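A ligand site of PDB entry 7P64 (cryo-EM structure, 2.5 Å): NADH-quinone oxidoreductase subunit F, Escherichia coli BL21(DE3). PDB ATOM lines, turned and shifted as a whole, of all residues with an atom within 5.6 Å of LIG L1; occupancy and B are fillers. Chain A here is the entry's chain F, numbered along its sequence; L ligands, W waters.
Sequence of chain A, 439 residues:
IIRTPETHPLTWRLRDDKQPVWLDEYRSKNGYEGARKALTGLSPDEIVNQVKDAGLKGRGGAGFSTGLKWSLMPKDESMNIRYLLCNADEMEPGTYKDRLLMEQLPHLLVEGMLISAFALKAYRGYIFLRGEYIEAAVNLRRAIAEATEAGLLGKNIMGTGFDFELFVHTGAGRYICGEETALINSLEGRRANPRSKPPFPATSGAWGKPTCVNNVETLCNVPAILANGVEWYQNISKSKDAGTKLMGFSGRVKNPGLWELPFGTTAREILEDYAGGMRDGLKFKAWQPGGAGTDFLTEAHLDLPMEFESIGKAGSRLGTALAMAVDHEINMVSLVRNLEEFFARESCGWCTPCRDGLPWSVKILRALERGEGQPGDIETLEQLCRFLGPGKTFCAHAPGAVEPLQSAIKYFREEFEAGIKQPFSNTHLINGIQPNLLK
The backbone carbonyl oxygen (O) of Asn 87 lies close to the side-chain amide oxygen (OD1) of Asn 215, at 3.2 Å. O of Gly 178 lies within hydrogen-bond range of ND2 of Asn 87, at 2.5 Å. N of Gly 60 sits close to ND2 of Asn 215 (3.4 Å). ND2 of Asn 215 sits at hydrogen-bond distance from O of Arg 59 (3.0 Å). NZ of Lys 69 sits close to ND2 of Asn 214, 3.4 Å away. The side-chain carboxylate (OE2) of Glu 90 lies within hydrogen-bond range of the backbone NH (N) of Asp 98, 2.5 Å away. The backbone NH (N) of Gly 178 sits at hydrogen-bond distance from the side-chain carboxylate (OD2) of Asp 89, at 3.0 Å. The side-chain carboxylate of Glu 92 lies within hydrogen-bond range of the side-chain hydroxyl of Tyr 175.
An oxygen (O5) of LIG L1 is in hydrogen-bond range of the side-chain amide nitrogen (ND2) of Asn 87 (2.5 Å). An oxygen (O7) of LIG L1 lies within hydrogen-bond range of the backbone NH (N) of Gly 60. The backbone NH (N) of Asn 215 sits at hydrogen-bond distance from an oxygen (O9) of LIG L1, 2.8 Å away. OD1 of Asn 215 sits close to O1 of LIG L1 (2.9 Å). An oxygen (O8) of LIG L1 is in salt-bridge range of the side-chain amino group of Lys 69, at 2.9 Å. An oxygen (O2) of LIG L1 sits at hydrogen-bond distance from the backbone NH (N) of Glu 90 (3.0 Å). The backbone NH (N) of Arg 59 lies within hydrogen-bond range of an oxygen (O7) of LIG L1 (3.4 Å). The backbone NH of Met 91 is in hydrogen-bond range of an oxygen (O2) of LIG L1 (3.4 Å). O3 of LIG L1 sits at hydrogen-bond distance from N of Glu 180. NZ of Lys 69 sits at hydrogen-bond distance from O5 of LG2 L2 (2.8 Å). The side-chain carboxylate (OE1) of Glu 180 lies within hydrogen-bond range of an oxygen (O5) of LG2 L2. An oxygen (O13) of LG2 L2 sits at hydrogen-bond distance from the backbone carbonyl oxygen (O) of Gly 61, 2.8 Å away.
An oxygen (O9) of LG2 L2 lies within hydrogen-bond range of an oxygen (O3) of LIG L1 (2.7 Å).
O of Gly 178 sits close to N4 of LIG L1 (3.4 Å). Merely in contact with LIG L1: Gly 58, Asp 89, Tyr 175, Ile 176, Glu 179, Val 213, Asn 214, Thr 218, Ala 396 and His 397.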
ATOM      1  N   LYS A  57     -36.660 -30.987 -34.239  1.00  0.00           N
ATOM      2  CA  LYS A  57     -36.002 -29.829 -33.650  1.00  0.00           C
ATOM      3  C   LYS A  57     -35.013 -30.275 -32.586  1.00  0.00           C
ATOM      4  O   LYS A  57     -34.999 -31.438 -32.152  1.00  0.00           O
ATOM      5  CB  LYS A  57     -37.034 -28.872 -33.052  1.00  0.00           C
ATOM      6  CG  LYS A  57     -37.892 -28.177 -34.095  1.00  0.00           C
ATOM      7  CD  LYS A  57     -38.906 -27.244 -33.451  1.00  0.00           C
ATOM      8  CE  LYS A  57     -39.630 -26.416 -34.489  1.00  0.00           C
ATOM      9  NZ  LYS A  57     -40.480 -27.253 -35.378  1.00  0.00           N
ATOM     10  N   GLY A  58     -34.167 -29.343 -32.165  1.00  0.00           N
ATOM     11  CA  GLY A  58     -33.148 -29.651 -31.178  1.00  0.00           C
ATOM     12  C   GLY A  58     -33.765 -29.928 -29.818  1.00  0.00           C
ATOM     13  O   GLY A  58     -34.529 -29.123 -29.284  1.00  0.00           O
ATOM     14  N   ARG A  59     -33.428 -31.078 -29.248  1.00  0.00           N
ATOM     15  CA  ARG A  59     -33.956 -31.487 -27.955  1.00  0.00           C
ATOM     16  C   ARG A  59     -33.073 -31.041 -26.791  1.00  0.00           C
ATOM     17  O   ARG A  59     -33.365 -31.382 -25.647  1.00  0.00           O
ATOM     18  CB  ARG A  59     -34.111 -33.012 -27.906  1.00  0.00           C
ATOM     19  CG  ARG A  59     -35.012 -33.561 -28.995  1.00  0.00           C
ATOM     20  CD  ARG A  59     -36.436 -33.089 -28.808  1.00  0.00           C
ATOM     21  NE  ARG A  59     -37.394 -33.940 -29.493  1.00  0.00           N
ATOM     22  CZ  ARG A  59     -38.032 -33.596 -30.605  1.00  0.00           C
ATOM     23  NH1 ARG A  59     -37.831 -32.426 -31.193  1.00  0.00           N
ATOM     24  NH2 ARG A  59     -38.902 -34.454 -31.140  1.00  0.00           N
ATOM     25  N   GLY A  60     -31.997 -30.290 -27.067  1.00  0.00           N
ATOM     26  CA  GLY A  60     -31.199 -29.743 -25.986  1.00  0.00           C
ATOM     27  C   GLY A  60     -31.953 -28.713 -25.169  1.00  0.00           C
ATOM     28  O   GLY A  60     -31.823 -28.657 -23.945  1.00  0.00           O
ATOM     29  N   GLY A  61     -32.772 -27.898 -25.829  1.00  0.00           N
ATOM     30  CA  GLY A  61     -33.523 -26.884 -25.131  1.00  0.00           C
ATOM     31  C   GLY A  61     -33.687 -25.611 -25.931  1.00  0.00           C
ATOM     32  O   GLY A  61     -34.423 -24.705 -25.528  1.00  0.00           O
ATOM     33  N   ALA A  62     -32.997 -25.518 -27.061  1.00  0.00           N
ATOM     34  CA  ALA A  62     -33.093 -24.345 -27.920  1.00  0.00           C
ATOM     35  C   ALA A  62     -34.088 -24.518 -29.055  1.00  0.00           C
ATOM     36  O   ALA A  62     -34.580 -23.504 -29.581  1.00  0.00           O
ATOM     37  CB  ALA A  62     -31.723 -24.006 -28.503  1.00  0.00           C
ATOM     38  N   GLY A  63     -34.405 -25.737 -29.453  1.00  0.00           N
ATOM     39  CA  GLY A  63     -35.411 -25.971 -30.472  1.00  0.00           C
ATOM     40  C   GLY A  63     -34.984 -25.681 -31.884  1.00  0.00           C
ATOM     41  O   GLY A  63     -35.850 -25.536 -32.751  1.00  0.00           O
ATOM     42  N   PHE A  64     -33.691 -25.561 -32.147  1.00  0.00           N
ATOM     43  CA  PHE A  64     -33.216 -25.351 -33.505  1.00  0.00           C
ATOM     44  C   PHE A  64     -33.431 -26.595 -34.350  1.00  0.00           C
ATOM     45  O   PHE A  64     -33.325 -27.716 -33.849  1.00  0.00           O
ATOM     46  CB  PHE A  64     -31.738 -24.960 -33.510  1.00  0.00           C
ATOM     47  CG  PHE A  64     -31.259 -24.376 -34.799  1.00  0.00           C
ATOM     48  CD1 PHE A  64     -31.533 -23.055 -35.128  1.00  0.00           C
ATOM     49  CD2 PHE A  64     -30.514 -25.139 -35.683  1.00  0.00           C
ATOM     50  CE1 PHE A  64     -31.089 -22.520 -36.313  1.00  0.00           C
ATOM     51  CE2 PHE A  64     -30.064 -24.598 -36.880  1.00  0.00           C
ATOM     52  CZ  PHE A  64     -30.349 -23.289 -37.185  1.00  0.00           C
ATOM     53  N   THR A  66     -32.925 -29.656 -36.670  1.00  0.00           N
ATOM     54  CA  THR A  66     -31.781 -30.535 -36.869  1.00  0.00           C
ATOM     55  C   THR A  66     -31.380 -30.587 -38.343  1.00  0.00           C
ATOM     56  O   THR A  66     -30.188 -30.577 -38.662  1.00  0.00           O
ATOM     57  CB  THR A  66     -32.108 -31.935 -36.367  1.00  0.00           C
ATOM     58  OG1 THR A  66     -32.764 -31.839 -35.091  1.00  0.00           O
ATOM     59  CG2 THR A  66     -30.840 -32.755 -36.214  1.00  0.00           C
ATOM     60  N   LYS A  69     -29.596 -27.380 -39.290  1.00  0.00           N
ATOM     61  CA  LYS A  69     -28.221 -27.394 -38.785  1.00  0.00           C
ATOM     62  C   LYS A  69     -27.343 -28.347 -39.596  1.00  0.00           C
ATOM     63  O   LYS A  69     -26.152 -28.070 -39.775  1.00  0.00           O
ATOM     64  CB  LYS A  69     -28.213 -27.787 -37.310  1.00  0.00           C
ATOM     65  CG  LYS A  69     -26.928 -27.466 -36.590  1.00  0.00           C
ATOM     66  CD  LYS A  69     -26.721 -28.375 -35.396  1.00  0.00           C
ATOM     67  CE  LYS A  69     -27.837 -28.224 -34.388  1.00  0.00           C
ATOM     68  NZ  LYS A  69     -27.457 -28.796 -33.076  1.00  0.00           N
ATOM     69  N   ASN A  87     -23.893 -34.531 -27.282  1.00  0.00           N
ATOM     70  CA  ASN A  87     -23.838 -33.777 -26.029  1.00  0.00           C
ATOM     71  C   ASN A  87     -24.568 -34.575 -24.953  1.00  0.00           C
ATOM     72  O   ASN A  87     -25.725 -34.324 -24.612  1.00  0.00           O
ATOM     73  CB  ASN A  87     -24.468 -32.401 -26.228  1.00  0.00           C
ATOM     74  CG  ASN A  87     -24.034 -31.412 -25.174  1.00  0.00           C
ATOM     75  OD1 ASN A  87     -23.635 -31.782 -24.080  1.00  0.00           O
ATOM     76  ND2 ASN A  87     -24.119 -30.126 -25.504  1.00  0.00           N
ATOM     77  N   ASP A  89     -23.675 -34.417 -21.919  1.00  0.00           N
ATOM     78  CA  ASP A  89     -23.249 -33.761 -20.678  1.00  0.00           C
ATOM     79  C   ASP A  89     -24.395 -33.713 -19.676  1.00  0.00           C
ATOM     80  O   ASP A  89     -24.296 -34.286 -18.588  1.00  0.00           O
ATOM     81  CB  ASP A  89     -22.739 -32.357 -20.978  1.00  0.00           C
ATOM     82  CG  ASP A  89     -21.554 -31.979 -20.116  1.00  0.00           C
ATOM     83  OD1 ASP A  89     -20.884 -32.890 -19.592  1.00  0.00           O
ATOM     84  OD2 ASP A  89     -21.289 -30.768 -19.954  1.00  0.00           O
ATOM     85  N   GLU A  90     -25.493 -33.036 -20.029  1.00  0.00           N
ATOM     86  CA  GLU A  90     -26.726 -32.988 -19.240  1.00  0.00           C
ATOM     87  C   GLU A  90     -26.481 -32.483 -17.820  1.00  0.00           C
ATOM     88  O   GLU A  90     -26.874 -33.102 -16.836  1.00  0.00           O
ATOM     89  CB  GLU A  90     -27.421 -34.354 -19.215  1.00  0.00           C
ATOM     90  CG  GLU A  90     -28.936 -34.269 -19.165  1.00  0.00           C
ATOM     91  CD  GLU A  90     -29.568 -35.518 -18.596  1.00  0.00           C
ATOM     92  OE1 GLU A  90     -28.904 -36.222 -17.806  1.00  0.00           O
ATOM     93  OE2 GLU A  90     -30.732 -35.807 -18.954  1.00  0.00           O
ATOM     94  N   MET A  91     -25.813 -31.334 -17.731  1.00  0.00           N
ATOM     95  CA  MET A  91     -25.408 -30.804 -16.437  1.00  0.00           C
ATOM     96  C   MET A  91     -26.417 -29.815 -15.855  1.00  0.00           C
ATOM     97  O   MET A  91     -26.174 -29.286 -14.770  1.00  0.00           O
ATOM     98  CB  MET A  91     -24.038 -30.135 -16.560  1.00  0.00           C
ATOM     99  CG  MET A  91     -22.898 -31.050 -16.170  1.00  0.00           C
ATOM    100  SD  MET A  91     -22.334 -30.775 -14.487  1.00  0.00           S
ATOM    101  CE  MET A  91     -20.931 -31.873 -14.424  1.00  0.00           C
ATOM    102  N   GLU A  92     -27.510 -29.568 -16.557  1.00  0.00           N
ATOM    103  CA  GLU A  92     -28.536 -28.656 -16.048  1.00  0.00           C
ATOM    104  C   GLU A  92     -29.256 -29.283 -14.861  1.00  0.00           C
ATOM    105  O   GLU A  92     -29.634 -30.457 -14.931  1.00  0.00           O
ATOM    106  CB  GLU A  92     -29.536 -28.309 -17.134  1.00  0.00           C
ATOM    107  CG  GLU A  92     -30.643 -27.369 -16.702  1.00  0.00           C
ATOM    108  CD  GLU A  92     -30.312 -25.924 -16.993  1.00  0.00           C
ATOM    109  OE1 GLU A  92     -29.374 -25.387 -16.369  1.00  0.00           O
ATOM    110  OE2 GLU A  92     -30.991 -25.310 -17.845  1.00  0.00           O
ATOM    111  N   ASP A  98     -31.338 -37.855 -20.341  1.00  0.00           N
ATOM    112  CA  ASP A  98     -30.287 -38.544 -21.080  1.00  0.00           C
ATOM    113  C   ASP A  98     -29.712 -39.700 -20.273  1.00  0.00           C
ATOM    114  O   ASP A  98     -29.252 -40.686 -20.863  1.00  0.00           O
ATOM    115  CB  ASP A  98     -29.183 -37.562 -21.470  1.00  0.00           C
ATOM    116  CG  ASP A  98     -29.703 -36.403 -22.295  1.00  0.00           C
ATOM    117  OD1 ASP A  98     -30.778 -36.554 -22.918  1.00  0.00           O
ATOM    118  OD2 ASP A  98     -29.030 -35.350 -22.339  1.00  0.00           O
ATOM    119  N   TYR A 175     -20.201 -27.405 -15.615  1.00  0.00           N
ATOM    120  CA  TYR A 175     -21.520 -27.208 -16.214  1.00  0.00           C
ATOM    121  C   TYR A 175     -21.427 -26.523 -17.581  1.00  0.00           C
ATOM    122  O   TYR A 175     -22.223 -26.838 -18.472  1.00  0.00           O
ATOM    123  CB  TYR A 175     -22.405 -26.389 -15.281  1.00  0.00           C
ATOM    124  CG  TYR A 175     -23.634 -25.792 -15.931  1.00  0.00           C
ATOM    125  CD1 TYR A 175     -24.731 -26.590 -16.231  1.00  0.00           C
ATOM    126  CD2 TYR A 175     -23.706 -24.437 -16.220  1.00  0.00           C
ATOM    127  CE1 TYR A 175     -25.858 -26.054 -16.813  1.00  0.00           C
ATOM    128  CE2 TYR A 175     -24.833 -23.901 -16.803  1.00  0.00           C
ATOM    129  CZ  TYR A 175     -25.898 -24.705 -17.092  1.00  0.00           C
ATOM    130  OH  TYR A 175     -27.017 -24.163 -17.676  1.00  0.00           O
ATOM    131  N   ILE A 176     -20.476 -25.611 -17.755  1.00  0.00           N
ATOM    132  CA  ILE A 176     -20.335 -24.876 -19.009  1.00  0.00           C
ATOM    133  C   ILE A 176     -19.913 -25.762 -20.172  1.00  0.00           C
ATOM    134  O   ILE A 176     -20.072 -25.366 -21.334  1.00  0.00           O
ATOM    135  CB  ILE A 176     -19.342 -23.708 -18.804  1.00  0.00           C
ATOM    136  CG1 ILE A 176     -19.559 -22.601 -19.848  1.00  0.00           C
ATOM    137  CG2 ILE A 176     -17.908 -24.200 -18.796  1.00  0.00           C
ATOM    138  CD1 ILE A 176     -20.993 -22.241 -20.096  1.00  0.00           C
ATOM    139  N   CYS A 177     -19.436 -26.985 -19.905  1.00  0.00           N
ATOM    140  CA  CYS A 177     -19.051 -27.913 -20.952  1.00  0.00           C
ATOM    141  C   CYS A 177     -20.228 -28.358 -21.819  1.00  0.00           C
ATOM    142  O   CYS A 177     -20.002 -28.903 -22.901  1.00  0.00           O
ATOM    143  CB  CYS A 177     -18.387 -29.153 -20.347  1.00  0.00           C
ATOM    144  SG  CYS A 177     -16.862 -28.824 -19.485  1.00  0.00           S
ATOM    145  N   GLY A 178     -21.465 -28.162 -21.370  1.00  0.00           N
ATOM    146  CA  GLY A 178     -22.605 -28.512 -22.182  1.00  0.00           C
ATOM    147  C   GLY A 178     -22.851 -27.574 -23.351  1.00  0.00           C
ATOM    148  O   GLY A 178     -23.474 -27.988 -24.325  1.00  0.00           O
ATOM    149  N   GLU A 179     -22.398 -26.327 -23.238  1.00  0.00           N
ATOM    150  CA  GLU A 179     -22.456 -25.409 -24.376  1.00  0.00           C
ATOM    151  C   GLU A 179     -21.590 -25.932 -25.509  1.00  0.00           C
ATOM    152  O   GLU A 179     -20.476 -26.405 -25.289  1.00  0.00           O
ATOM    153  CB  GLU A 179     -21.975 -24.019 -23.949  1.00  0.00           C
ATOM    154  CG  GLU A 179     -22.608 -22.874 -24.718  1.00  0.00           C
ATOM    155  CD  GLU A 179     -21.778 -22.441 -25.919  1.00  0.00           C
ATOM    156  OE1 GLU A 179     -20.606 -22.835 -25.998  1.00  0.00           O
ATOM    157  OE2 GLU A 179     -22.314 -21.711 -26.771  1.00  0.00           O
ATOM    158  N   GLU A 180     -22.120 -25.855 -26.733  1.00  0.00           N
ATOM    159  CA  GLU A 180     -21.561 -26.601 -27.861  1.00  0.00           C
ATOM    160  C   GLU A 180     -20.136 -26.168 -28.204  1.00  0.00           C
ATOM    161  O   GLU A 180     -19.270 -27.018 -28.458  1.00  0.00           O
ATOM    162  CB  GLU A 180     -22.467 -26.475 -29.084  1.00  0.00           C
ATOM    163  CG  GLU A 180     -22.783 -25.053 -29.479  1.00  0.00           C
ATOM    164  CD  GLU A 180     -23.395 -24.941 -30.853  1.00  0.00           C
ATOM    165  OE1 GLU A 180     -23.604 -25.990 -31.500  1.00  0.00           O
ATOM    166  OE2 GLU A 180     -23.621 -23.804 -31.292  1.00  0.00           O
ATOM    167  N   VAL A 213     -22.893 -30.797 -33.478  1.00  0.00           N
ATOM    168  CA  VAL A 213     -23.166 -31.174 -32.100  1.00  0.00           C
ATOM    169  C   VAL A 213     -24.666 -31.343 -31.930  1.00  0.00           C
ATOM    170  O   VAL A 213     -25.443 -30.439 -32.272  1.00  0.00           O
ATOM    171  CB  VAL A 213     -22.628 -30.126 -31.108  1.00  0.00           C
ATOM    172  CG1 VAL A 213     -22.777 -30.619 -29.681  1.00  0.00           C
ATOM    173  CG2 VAL A 213     -21.175 -29.792 -31.424  1.00  0.00           C
ATOM    174  N   ASN A 214     -25.079 -32.497 -31.418  1.00  0.00           N
ATOM    175  CA  ASN A 214     -26.502 -32.773 -31.205  1.00  0.00           C
ATOM    176  C   ASN A 214     -26.708 -33.429 -29.852  1.00  0.00           C
ATOM    177  O   ASN A 214     -25.822 -34.115 -29.334  1.00  0.00           O
ATOM    178  CB  ASN A 214     -27.073 -33.666 -32.315  1.00  0.00           C
ATOM    179  CG  ASN A 214     -27.327 -32.922 -33.597  1.00  0.00           C
ATOM    180  OD1 ASN A 214     -26.646 -33.135 -34.601  1.00  0.00           O
ATOM    181  ND2 ASN A 214     -28.309 -32.024 -33.576  1.00  0.00           N
ATOM    182  N   ASN A 215     -27.892 -33.228 -29.293  1.00  0.00           N
ATOM    183  CA  ASN A 215     -28.259 -33.812 -28.010  1.00  0.00           C
ATOM    184  C   ASN A 215     -28.485 -35.318 -28.157  1.00  0.00           C
ATOM    185  O   ASN A 215     -28.592 -35.852 -29.265  1.00  0.00           O
ATOM    186  CB  ASN A 215     -29.512 -33.130 -27.457  1.00  0.00           C
ATOM    187  CG  ASN A 215     -29.708 -33.362 -25.981  1.00  0.00           C
ATOM    188  OD1 ASN A 215     -28.806 -33.840 -25.290  1.00  0.00           O
ATOM    189  ND2 ASN A 215     -30.892 -33.061 -25.481  1.00  0.00           N
ATOM    190  N   VAL A 216     -28.527 -36.008 -27.017  1.00  0.00           N
ATOM    191  CA  VAL A 216     -28.834 -37.440 -26.997  1.00  0.00           C
ATOM    192  C   VAL A 216     -30.234 -37.701 -27.529  1.00  0.00           C
ATOM    193  O   VAL A 216     -30.447 -38.628 -28.326  1.00  0.00           O
ATOM    194  CB  VAL A 216     -28.674 -37.999 -25.581  1.00  0.00           C
ATOM    195  CG1 VAL A 216     -28.871 -39.501 -25.579  1.00  0.00           C
ATOM    196  CG2 VAL A 216     -27.326 -37.633 -25.016  1.00  0.00           C
ATOM    197  N   THR A 218     -32.174 -35.916 -29.541  1.00  0.00           N
ATOM    198  CA  THR A 218     -32.297 -35.681 -30.976  1.00  0.00           C
ATOM    199  C   THR A 218     -31.787 -36.873 -31.772  1.00  0.00           C
ATOM    200  O   THR A 218     -32.453 -37.364 -32.694  1.00  0.00           O
ATOM    201  CB  THR A 218     -31.534 -34.419 -31.366  1.00  0.00           C
ATOM    202  OG1 THR A 218     -31.957 -33.321 -30.550  1.00  0.00           O
ATOM    203  CG2 THR A 218     -31.757 -34.072 -32.824  1.00  0.00           C
ATOM    204  N   CYS A 395     -21.797 -15.675 -23.818  1.00  0.00           N
ATOM    205  CA  CYS A 395     -22.581 -16.863 -24.135  1.00  0.00           C
ATOM    206  C   CYS A 395     -23.908 -16.777 -23.398  1.00  0.00           C
ATOM    207  O   CYS A 395     -24.209 -15.783 -22.723  1.00  0.00           O
ATOM    208  CB  CYS A 395     -21.805 -18.134 -23.789  1.00  0.00           C
ATOM    209  SG  CYS A 395     -22.070 -18.783 -22.142  1.00  0.00           S
ATOM    210  N   ALA A 396     -24.716 -17.821 -23.531  1.00  0.00           N
ATOM    211  CA  ALA A 396     -26.092 -17.822 -23.045  1.00  0.00           C
ATOM    212  C   ALA A 396     -26.226 -18.361 -21.636  1.00  0.00           C
ATOM    213  O   ALA A 396     -27.354 -18.597 -21.181  1.00  0.00           O
ATOM    214  CB  ALA A 396     -26.980 -18.631 -23.994  1.00  0.00           C
ATOM    215  N   HIS A 397     -25.111 -18.584 -20.929  1.00  0.00           N
ATOM    216  CA  HIS A 397     -25.194 -19.090 -19.567  1.00  0.00           C
ATOM    217  C   HIS A 397     -25.774 -18.055 -18.618  1.00  0.00           C
ATOM    218  O   HIS A 397     -26.609 -18.377 -17.768  1.00  0.00           O
ATOM    219  CB  HIS A 397     -23.803 -19.533 -19.109  1.00  0.00           C
ATOM    220  CG  HIS A 397     -23.644 -19.624 -17.627  1.00  0.00           C
ATOM    221  ND1 HIS A 397     -23.175 -18.587 -16.856  1.00  0.00           N
ATOM    222  CD2 HIS A 397     -23.883 -20.647 -16.766  1.00  0.00           C
ATOM    223  CE1 HIS A 397     -23.135 -18.952 -15.590  1.00  0.00           C
ATOM    224  NE2 HIS A 397     -23.552 -20.204 -15.504  1.00  0.00           N
HETATM  225  N1  LIG L   1     -27.131 -29.144 -24.515  1.00  0.00           N
HETATM  226  C1  LIG L   1     -27.105 -30.468 -24.135  1.00  0.00           C
HETATM  227  O1  LIG L   1     -27.524 -31.313 -24.914  1.00  0.00           O
HETATM  228  N2  LIG L   1     -26.615 -30.825 -22.913  1.00  0.00           N
HETATM  229  C2  LIG L   1     -26.136 -29.854 -22.053  1.00  0.00           C
HETATM  230  O2  LIG L   1     -25.698 -30.174 -20.959  1.00  0.00           O
HETATM  231  C3  LIG L   1     -26.167 -28.521 -22.430  1.00  0.00           C
HETATM  232  N3  LIG L   1     -25.695 -27.549 -21.589  1.00  0.00           N
HETATM  233  C4  LIG L   1     -25.720 -26.225 -21.969  1.00  0.00           C
HETATM  234  C5  LIG L   1     -25.238 -25.268 -21.090  1.00  0.00           C
HETATM  235  C6  LIG L   1     -25.263 -23.923 -21.458  1.00  0.00           C
HETATM  236  C7  LIG L   1     -24.740 -22.901 -20.495  1.00  0.00           C
HETATM  237  C8  LIG L   1     -25.765 -23.556 -22.698  1.00  0.00           C
HETATM  238  C9  LIG L   1     -25.792 -22.117 -23.103  1.00  0.00           C
HETATM  239  C10 LIG L   1     -26.239 -24.522 -23.569  1.00  0.00           C
HETATM  240  C11 LIG L   1     -26.217 -25.867 -23.211  1.00  0.00           C
HETATM  241  N4  LIG L   1     -26.690 -26.847 -24.073  1.00  0.00           N
HETATM  242  C12 LIG L   1     -26.664 -28.163 -23.672  1.00  0.00           C
HETATM  243  C13 LIG L   1     -27.246 -26.508 -25.433  1.00  0.00           C
HETATM  244  C14 LIG L   1     -26.132 -26.601 -26.480  1.00  0.00           C
HETATM  245  O3  LIG L   1     -25.567 -25.328 -26.656  1.00  0.00           O
HETATM  246  C15 LIG L   1     -26.635 -27.121 -27.825  1.00  0.00           C
HETATM  247  O4  LIG L   1     -27.822 -26.449 -28.192  1.00  0.00           O
HETATM  248  C16 LIG L   1     -26.884 -28.620 -27.775  1.00  0.00           C
HETATM  249  O5  LIG L   1     -25.796 -29.249 -27.164  1.00  0.00           O
HETATM  250  C17 LIG L   1     -27.105 -29.244 -29.146  1.00  0.00           C
HETATM  251  O6  LIG L   1     -28.194 -28.623 -29.778  1.00  0.00           O
HETATM  252  P1  LIG L   1     -29.468 -29.490 -30.244  1.00  0.00           P
HETATM  253  O7  LIG L   1     -30.535 -29.326 -29.209  1.00  0.00           O
HETATM  254  O8  LIG L   1     -29.951 -28.999 -31.589  1.00  0.00           O
HETATM  255  O9  LIG L   1     -29.106 -30.948 -30.340  1.00  0.00           O
HETATM  256  P1  LG2 L   2     -28.509 -21.194 -29.688  1.00  0.00           P
HETATM  257  O1  LG2 L   2     -29.957 -21.306 -29.416  1.00  0.00           O
HETATM  258  O2  LG2 L   2     -28.104 -19.985 -30.521  1.00  0.00           O
HETATM  259  O3  LG2 L   2     -27.966 -22.493 -30.458  1.00  0.00           O
HETATM  260  C1  LG2 L   2     -28.621 -23.772 -30.389  1.00  0.00           C
HETATM  261  C2  LG2 L   2     -28.284 -24.571 -31.626  1.00  0.00           C
HETATM  262  O4  LG2 L   2     -28.701 -23.838 -32.801  1.00  0.00           O
HETATM  263  C3  LG2 L   2     -26.804 -24.888 -31.803  1.00  0.00           C
HETATM  264  O5  LG2 L   2     -26.596 -26.269 -32.108  1.00  0.00           O
HETATM  265  C4  LG2 L   2     -26.372 -23.969 -32.954  1.00  0.00           C
HETATM  266  O6  LG2 L   2     -25.357 -24.566 -33.761  1.00  0.00           O
HETATM  267  C5  LG2 L   2     -27.666 -23.837 -33.754  1.00  0.00           C
HETATM  268  N1  LG2 L   2     -27.755 -22.599 -34.517  1.00  0.00           N
HETATM  269  C6  LG2 L   2     -28.494 -21.485 -34.219  1.00  0.00           C
HETATM  270  N2  LG2 L   2     -28.384 -20.517 -35.093  1.00  0.00           N
HETATM  271  C7  LG2 L   2     -27.507 -21.032 -36.040  1.00  0.00           C
HETATM  272  C8  LG2 L   2     -26.963 -20.495 -37.226  1.00  0.00           C
HETATM  273  N3  LG2 L   2     -27.268 -19.277 -37.698  1.00  0.00           N
HETATM  274  N4  LG2 L   2     -26.111 -21.261 -37.924  1.00  0.00           N
HETATM  275  C9  LG2 L   2     -25.808 -22.478 -37.462  1.00  0.00           C
HETATM  276  N5  LG2 L   2     -26.252 -23.086 -36.365  1.00  0.00           N
HETATM  277  C10 LG2 L   2     -27.103 -22.312 -35.688  1.00  0.00           C
HETATM  278  O7  LG2 L   2     -27.662 -21.135 -28.341  1.00  0.00           O
HETATM  279  P2  LG2 L   2     -26.953 -22.220 -27.426  1.00  0.00           P
HETATM  280  O8  LG2 L   2     -26.091 -21.470 -26.409  1.00  0.00           O
HETATM  281  O9  LG2 L   2     -26.214 -23.219 -28.215  1.00  0.00           O
HETATM  282  O10 LG2 L   2     -28.144 -22.899 -26.593  1.00  0.00           O
HETATM  283  C11 LG2 L   2     -28.909 -22.160 -25.619  1.00  0.00           C
HETATM  284  C12 LG2 L   2     -30.016 -23.054 -25.108  1.00  0.00           C
HETATM  285  O11 LG2 L   2     -29.446 -24.181 -24.424  1.00  0.00           O
HETATM  286  C13 LG2 L   2     -30.926 -22.401 -24.069  1.00  0.00           C
HETATM  287  O12 LG2 L   2     -32.013 -21.730 -24.700  1.00  0.00           O
HETATM  288  C14 LG2 L   2     -31.403 -23.589 -23.212  1.00  0.00           C
HETATM  289  O13 LG2 L   2     -32.760 -23.919 -23.466  1.00  0.00           O
HETATM  290  C15 LG2 L   2     -30.468 -24.734 -23.608  1.00  0.00           C
HETATM  291  N6  LG2 L   2     -29.844 -25.398 -22.466  1.00  0.00           N
HETATM  292  C16 LG2 L   2     -29.836 -26.794 -22.368  1.00  0.00           C
HETATM  293  C17 LG2 L   2     -29.284 -27.453 -21.328  1.00  0.00           C
HETATM  294  C18 LG2 L   2     -29.346 -28.938 -21.339  1.00  0.00           C
HETATM  295  O14 LG2 L   2     -29.613 -29.542 -22.388  1.00  0.00           O
HETATM  296  N7  LG2 L   2     -29.105 -29.566 -20.206  1.00  0.00           N
HETATM  297  C19 LG2 L   2     -28.637 -26.697 -20.208  1.00  0.00           C
HETATM  298  C20 LG2 L   2     -28.680 -25.231 -20.427  1.00  0.00           C
HETATM  299  C21 LG2 L   2     -29.240 -24.671 -21.480  1.00  0.00           C
HETATM  300  O   HOH W   1     -26.892 -33.618 -22.548  1.00  0.00           O
